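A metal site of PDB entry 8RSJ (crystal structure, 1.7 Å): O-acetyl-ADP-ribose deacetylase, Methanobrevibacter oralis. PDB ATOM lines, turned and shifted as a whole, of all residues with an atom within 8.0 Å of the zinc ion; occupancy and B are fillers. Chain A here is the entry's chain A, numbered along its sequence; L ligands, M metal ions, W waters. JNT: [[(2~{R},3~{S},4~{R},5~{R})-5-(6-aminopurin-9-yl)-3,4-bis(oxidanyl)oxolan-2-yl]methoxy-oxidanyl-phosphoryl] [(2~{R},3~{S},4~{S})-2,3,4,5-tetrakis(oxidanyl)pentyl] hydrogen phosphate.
The side-chain carboxylate (OD2) of Asp 118 lies within hydrogen-bond range of an oxygen (O1C) of the ligand (2.6 Å).
The backbone NH (N) of Ile 117 is in hydrogen-bond range of an oxygen (O1A) of the ligand.
The side-chain amide nitrogen of Asn 103 lies within hydrogen-bond range of an oxygen (O1C) of the ligand (2.9 Å).
The backbone NH (N) of Val 212 sits at hydrogen-bond distance from an oxygen (O2A) of the ligand (3.0 Å).
The side-chain sulfur (SG) of Cys 109 lies close to the backbone NH (N) of Ile 111 (3.5 Å).
The side-chain sulfur of Cys 116 sits close to the backbone NH of Asp 118.
SG of Cys 116 sits close to N of Asn 119, 3.2 Å away.
SG of Cys 109 lies close to ND2 of Asn 119 (3.5 Å).
NH2 of Arg 38 sits at hydrogen-bond distance from O of His 114, at 3.0 Å.
OD1 of Asn 119 lies close to O of His 114, 3.3 Å away.
Water W1 binds the zinc ion (2.0 Å).
ND1 of His 114 binds the zinc ion (2.1 Å).
The zinc ion is bound by SG of Cys 116 (2.3 Å).
The zinc ion is bound by the side-chain sulfur (SG) of Cys 109.
The zinc ion has four donor atoms within binding distance.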
ATOM      1  N   ARG A  38      -1.293  23.147 -30.440  1.00  0.00           N
ATOM      2  CA  ARG A  38      -1.747  23.226 -29.058  1.00  0.00           C
ATOM      3  C   ARG A  38      -3.294  23.150 -28.912  1.00  0.00           C
ATOM      4  O   ARG A  38      -3.809  22.410 -28.060  1.00  0.00           O
ATOM      5  CB  ARG A  38      -1.171  24.466 -28.374  1.00  0.00           C
ATOM      6  CG  ARG A  38      -1.608  24.609 -26.922  1.00  0.00           C
ATOM      7  CD  ARG A  38      -0.945  25.834 -26.284  1.00  0.00           C
ATOM      8  NE  ARG A  38      -1.647  26.277 -25.106  1.00  0.00           N
ATOM      9  CZ  ARG A  38      -1.494  27.453 -24.537  1.00  0.00           C
ATOM     10  NH1 ARG A  38      -0.653  28.321 -25.058  1.00  0.00           N
ATOM     11  NH2 ARG A  38      -2.180  27.738 -23.444  1.00  0.00           N
ATOM     12  N   ASN A  42      -5.344  20.415 -26.941  1.00  0.00           N
ATOM     13  CA  ASN A  42      -6.265  20.850 -25.883  1.00  0.00           C
ATOM     14  C   ASN A  42      -7.647  20.201 -26.004  1.00  0.00           C
ATOM     15  O   ASN A  42      -8.184  19.733 -25.018  1.00  0.00           O
ATOM     16  CB  ASN A  42      -6.436  22.389 -25.832  1.00  0.00           C
ATOM     17  CG  ASN A  42      -5.207  23.196 -25.487  1.00  0.00           C
ATOM     18  OD1 ASN A  42      -5.169  24.379 -25.800  1.00  0.00           O
ATOM     19  ND2 ASN A  42      -4.193  22.596 -24.888  1.00  0.00           N
ATOM     20  N   ALA A 101      -2.371  22.729 -10.782  1.00  0.00           N
ATOM     21  CA  ALA A 101      -3.704  23.064 -10.299  1.00  0.00           C
ATOM     22  C   ALA A 101      -4.730  22.559 -11.318  1.00  0.00           C
ATOM     23  O   ALA A 101      -5.132  23.234 -12.250  1.00  0.00           O
ATOM     24  CB  ALA A 101      -3.838  24.529 -10.050  1.00  0.00           C
ATOM     25  N   ASN A 103      -8.296  20.403 -12.689  1.00  0.00           N
ATOM     26  CA  ASN A 103      -9.737  20.437 -12.383  1.00  0.00           C
ATOM     27  C   ASN A 103     -10.152  19.056 -11.889  1.00  0.00           C
ATOM     28  O   ASN A 103      -9.394  18.093 -12.107  1.00  0.00           O
ATOM     29  CB  ASN A 103     -10.630  20.972 -13.510  1.00  0.00           C
ATOM     30  CG  ASN A 103     -10.472  20.228 -14.811  1.00  0.00           C
ATOM     31  OD1 ASN A 103     -10.797  19.052 -14.843  1.00  0.00           O
ATOM     32  ND2 ASN A 103      -9.948  20.871 -15.837  1.00  0.00           N
ATOM     33  N   GLY A 108      -7.021  17.722 -17.747  1.00  0.00           N
ATOM     34  CA  GLY A 108      -6.488  18.940 -18.294  1.00  0.00           C
ATOM     35  C   GLY A 108      -7.611  19.869 -18.771  1.00  0.00           C
ATOM     36  O   GLY A 108      -8.751  19.815 -18.316  1.00  0.00           O
ATOM     37  N   CYS A 109      -7.201  20.778 -19.665  1.00  0.00           N
ATOM     38  CA  CYS A 109      -8.072  21.869 -20.067  1.00  0.00           C
ATOM     39  C   CYS A 109      -8.400  21.687 -21.541  1.00  0.00           C
ATOM     40  O   CYS A 109      -7.503  21.588 -22.370  1.00  0.00           O
ATOM     41  CB  CYS A 109      -7.305  23.158 -19.858  1.00  0.00           C
ATOM     42  SG  CYS A 109      -8.173  24.594 -20.510  1.00  0.00           S
ATOM     43  N   PHE A 110      -9.690  21.701 -21.856  1.00  0.00           N
ATOM     44  CA  PHE A 110     -10.164  21.551 -23.213  1.00  0.00           C
ATOM     45  C   PHE A 110     -10.484  22.863 -23.905  1.00  0.00           C
ATOM     46  O   PHE A 110     -10.989  22.820 -25.033  1.00  0.00           O
ATOM     47  CB  PHE A 110     -11.370  20.633 -23.251  1.00  0.00           C
ATOM     48  CG  PHE A 110     -10.994  19.226 -22.887  1.00  0.00           C
ATOM     49  CD1 PHE A 110     -10.752  18.881 -21.565  1.00  0.00           C
ATOM     50  CD2 PHE A 110     -10.819  18.255 -23.864  1.00  0.00           C
ATOM     51  CE1 PHE A 110     -10.408  17.582 -21.229  1.00  0.00           C
ATOM     52  CE2 PHE A 110     -10.473  16.957 -23.519  1.00  0.00           C
ATOM     53  CZ  PHE A 110     -10.310  16.611 -22.202  1.00  0.00           C
ATOM     54  N   ILE A 111     -10.246  23.978 -23.242  1.00  0.00           N
ATOM     55  CA  ILE A 111     -10.526  25.281 -23.848  1.00  0.00           C
ATOM     56  C   ILE A 111      -9.273  25.627 -24.629  1.00  0.00           C
ATOM     57  O   ILE A 111      -8.310  25.776 -24.003  1.00  0.00           O
ATOM     58  CB  ILE A 111     -10.796  26.326 -22.769  1.00  0.00           C
ATOM     59  CG1 ILE A 111     -11.983  25.927 -21.892  1.00  0.00           C
ATOM     60  CG2 ILE A 111     -10.900  27.710 -23.419  1.00  0.00           C
ATOM     61  CD1 ILE A 111     -12.185  26.770 -20.688  1.00  0.00           C
ATOM     62  N   PRO A 112      -9.274  25.730 -25.976  1.00  0.00           N
ATOM     63  CA  PRO A 112      -8.060  25.947 -26.764  1.00  0.00           C
ATOM     64  C   PRO A 112      -7.375  27.256 -26.418  1.00  0.00           C
ATOM     65  O   PRO A 112      -8.067  28.251 -26.227  1.00  0.00           O
ATOM     66  CB  PRO A 112      -8.466  25.954 -28.236  1.00  0.00           C
ATOM     67  CG  PRO A 112      -9.979  25.921 -28.236  1.00  0.00           C
ATOM     68  CD  PRO A 112     -10.469  25.624 -26.819  1.00  0.00           C
ATOM     69  N   MET A 113      -6.050  27.146 -26.169  1.00  0.00           N
ATOM     70  CA  MET A 113      -5.169  28.296 -25.964  1.00  0.00           C
ATOM     71  C   MET A 113      -5.406  28.945 -24.594  1.00  0.00           C
ATOM     72  O   MET A 113      -4.918  30.045 -24.327  1.00  0.00           O
ATOM     73  CB  MET A 113      -5.314  29.383 -27.051  1.00  0.00           C
ATOM     74  CG  MET A 113      -4.915  28.977 -28.462  1.00  0.00           C
ATOM     75  SD  MET A 113      -3.263  28.268 -28.590  1.00  0.00           S
ATOM     76  CE  MET A 113      -3.755  26.629 -28.109  1.00  0.00           C
ATOM     77  N   HIS A 114      -6.085  28.260 -23.666  1.00  0.00           N
ATOM     78  CA  HIS A 114      -6.384  28.873 -22.383  1.00  0.00           C
ATOM     79  C   HIS A 114      -5.113  28.879 -21.542  1.00  0.00           C
ATOM     80  O   HIS A 114      -4.415  27.860 -21.516  1.00  0.00           O
ATOM     81  CB  HIS A 114      -7.475  28.054 -21.665  1.00  0.00           C
ATOM     82  CG  HIS A 114      -8.123  28.767 -20.522  1.00  0.00           C
ATOM     83  ND1 HIS A 114      -8.441  28.058 -19.383  1.00  0.00           N
ATOM     84  CD2 HIS A 114      -8.512  30.058 -20.253  1.00  0.00           C
ATOM     85  CE1 HIS A 114      -9.052  28.838 -18.523  1.00  0.00           C
ATOM     86  NE2 HIS A 114      -8.994  30.112 -18.995  1.00  0.00           N
ATOM     87  N   ASN A 115      -4.796  30.037 -20.931  1.00  0.00           N
ATOM     88  CA  ASN A 115      -3.514  30.138 -20.248  1.00  0.00           C
ATOM     89  C   ASN A 115      -3.623  29.848 -18.752  1.00  0.00           C
ATOM     90  O   ASN A 115      -2.758  30.271 -17.979  1.00  0.00           O
ATOM     91  CB  ASN A 115      -2.755  31.415 -20.632  1.00  0.00           C
ATOM     92  CG  ASN A 115      -2.292  31.472 -22.084  1.00  0.00           C
ATOM     93  OD1 ASN A 115      -1.639  30.566 -22.618  1.00  0.00           O
ATOM     94  ND2 ASN A 115      -2.562  32.593 -22.741  1.00  0.00           N
ATOM     95  N   CYS A 116      -4.570  28.955 -18.351  1.00  0.00           N
ATOM     96  CA  CYS A 116      -4.493  28.349 -17.025  1.00  0.00           C
ATOM     97  C   CYS A 116      -3.230  27.460 -16.962  1.00  0.00           C
ATOM     98  O   CYS A 116      -2.705  26.949 -17.984  1.00  0.00           O
ATOM     99  CB  CYS A 116      -5.778  27.569 -16.727  1.00  0.00           C
ATOM    100  SG  CYS A 116      -5.854  26.072 -17.762  1.00  0.00           S
ATOM    101  N   ILE A 117      -2.695  27.230 -15.753  1.00  0.00           N
ATOM    102  CA  ILE A 117      -1.474  26.428 -15.630  1.00  0.00           C
ATOM    103  C   ILE A 117      -1.724  24.985 -16.084  1.00  0.00           C
ATOM    104  O   ILE A 117      -0.836  24.316 -16.592  1.00  0.00           O
ATOM    105  CB  ILE A 117      -0.870  26.479 -14.214  1.00  0.00           C
ATOM    106  CG1 ILE A 117       0.644  26.227 -14.301  1.00  0.00           C
ATOM    107  CG2 ILE A 117      -1.606  25.532 -13.220  1.00  0.00           C
ATOM    108  CD1 ILE A 117       1.329  26.296 -12.996  1.00  0.00           C
ATOM    109  N   ASP A 118      -2.979  24.483 -15.940  1.00  0.00           N
ATOM    110  CA  ASP A 118      -3.351  23.124 -16.351  1.00  0.00           C
ATOM    111  C   ASP A 118      -3.135  22.930 -17.867  1.00  0.00           C
ATOM    112  O   ASP A 118      -2.514  21.949 -18.293  1.00  0.00           O
ATOM    113  CB  ASP A 118      -4.788  22.903 -15.879  1.00  0.00           C
ATOM    114  CG  ASP A 118      -5.337  21.496 -16.043  1.00  0.00           C
ATOM    115  OD1 ASP A 118      -4.567  20.561 -16.104  1.00  0.00           O
ATOM    116  OD2 ASP A 118      -6.527  21.368 -16.196  1.00  0.00           O
ATOM    117  N   ASN A 119      -3.639  23.870 -18.649  1.00  0.00           N
ATOM    118  CA  ASN A 119      -3.519  23.833 -20.095  1.00  0.00           C
ATOM    119  C   ASN A 119      -2.036  23.910 -20.475  1.00  0.00           C
ATOM    120  O   ASN A 119      -1.564  23.190 -21.337  1.00  0.00           O
ATOM    121  CB  ASN A 119      -4.298  24.971 -20.716  1.00  0.00           C
ATOM    122  CG  ASN A 119      -4.382  24.942 -22.226  1.00  0.00           C
ATOM    123  OD1 ASN A 119      -3.346  25.027 -22.900  1.00  0.00           O
ATOM    124  ND2 ASN A 119      -5.590  24.984 -22.767  1.00  0.00           N
ATOM    125  N   ILE A 120      -1.317  24.824 -19.829  1.00  0.00           N
ATOM    126  CA  ILE A 120       0.086  25.041 -20.129  1.00  0.00           C
ATOM    127  C   ILE A 120       0.925  23.795 -19.845  1.00  0.00           C
ATOM    128  O   ILE A 120       1.809  23.419 -20.646  1.00  0.00           O
ATOM    129  CB  ILE A 120       0.561  26.283 -19.375  1.00  0.00           C
ATOM    130  CG1 ILE A 120      -0.127  27.468 -20.061  1.00  0.00           C
ATOM    131  CG2 ILE A 120       2.080  26.383 -19.313  1.00  0.00           C
ATOM    132  CD1 ILE A 120       0.249  28.794 -19.585  1.00  0.00           C
ATOM    133  N   VAL A 212      -7.562  31.918 -11.445  1.00  0.00           N
ATOM    134  CA  VAL A 212      -8.989  32.003 -11.703  1.00  0.00           C
ATOM    135  C   VAL A 212      -9.776  31.619 -10.463  1.00  0.00           C
ATOM    136  O   VAL A 212     -10.934  31.964 -10.365  1.00  0.00           O
ATOM    137  CB  VAL A 212      -9.411  31.159 -12.929  1.00  0.00           C
ATOM    138  CG1 VAL A 212      -9.310  29.654 -12.704  1.00  0.00           C
ATOM    139  CG2 VAL A 212     -10.815  31.507 -13.420  1.00  0.00           C
HETATM  140  O5' JNT L   1      -3.468  29.663 -11.469  1.00  0.00           O
HETATM  141  C5' JNT L   1      -2.699  28.924 -10.558  1.00  0.00           C
HETATM  142  C4' JNT L   1      -1.341  29.785 -10.430  1.00  0.00           C
HETATM  143  O4' JNT L   1      -0.498  29.363 -11.535  1.00  0.00           O
HETATM  144  C3' JNT L   1      -1.482  31.358 -10.522  1.00  0.00           C
HETATM  145  O3' JNT L   1      -0.584  31.940  -9.560  1.00  0.00           O
HETATM  146  C2' JNT L   1      -0.975  31.555 -11.960  1.00  0.00           C
HETATM  147  O2' JNT L   1      -0.460  32.865 -12.218  1.00  0.00           O
HETATM  148  C1' JNT L   1       0.132  30.652 -12.018  1.00  0.00           C
HETATM  149  N9  JNT L   1       0.581  30.269 -13.381  1.00  0.00           N
HETATM  150  C8  JNT L   1       0.013  30.333 -14.603  1.00  0.00           C
HETATM  151  N7  JNT L   1       0.891  29.859 -15.514  1.00  0.00           N
HETATM  152  C5  JNT L   1       1.990  29.500 -14.860  1.00  0.00           C
HETATM  153  C4  JNT L   1       1.788  29.757 -13.539  1.00  0.00           C
HETATM  154  N3  JNT L   1       2.757  29.498 -12.627  1.00  0.00           N
HETATM  155  C2  JNT L   1       3.965  28.965 -13.039  1.00  0.00           C
HETATM  156  N1  JNT L   1       4.169  28.733 -14.343  1.00  0.00           N
HETATM  157  C6  JNT L   1       3.209  28.987 -15.257  1.00  0.00           C
HETATM  158  N6  JNT L   1       3.445  28.682 -16.578  1.00  0.00           N
HETATM  159  O1C JNT L   1      -8.312  23.268 -16.114  1.00  0.00           O
HETATM  160  C1A JNT L   1      -8.005  23.751 -14.993  1.00  0.00           C
HETATM  161  C2A JNT L   1      -9.024  24.164 -13.924  1.00  0.00           C
HETATM  162  O2C JNT L   1     -10.128  24.684 -14.351  1.00  0.00           O
HETATM  163  C3A JNT L   1      -8.554  24.609 -12.542  1.00  0.00           C
HETATM  164  O3C JNT L   1      -9.571  24.041 -11.645  1.00  0.00           O
HETATM  165  C4A JNT L   1      -8.331  26.164 -12.344  1.00  0.00           C
HETATM  166  O4C JNT L   1      -7.317  26.719 -13.310  1.00  0.00           O
HETATM  167  C5A JNT L   1      -7.874  26.244 -10.882  1.00  0.00           C
HETATM  168  O5A JNT L   1      -7.660  27.667 -10.542  1.00  0.00           O
HETATM  169  PB  JNT L   1      -6.211  28.089 -10.046  1.00  0.00           P
HETATM  170  O2B JNT L   1      -6.401  29.611  -9.588  1.00  0.00           O
HETATM  171  O1B JNT L   1      -5.762  27.234  -8.976  1.00  0.00           O
HETATM  172  O3A JNT L   1      -5.258  27.958 -11.333  1.00  0.00           O
HETATM  173  PA  JNT L   1      -4.658  29.009 -12.375  1.00  0.00           P
HETATM  174  O1A JNT L   1      -4.038  28.063 -13.422  1.00  0.00           O
HETATM  175  O2A JNT L   1      -5.661  30.033 -12.784  1.00  0.00           O
HETATM  176 ZN    ZN M   1      -7.896  26.175 -18.775  1.00  0.00          ZN
HETATM  177  O   HOH W   1      -9.128  25.607 -17.323  1.00  0.00           O
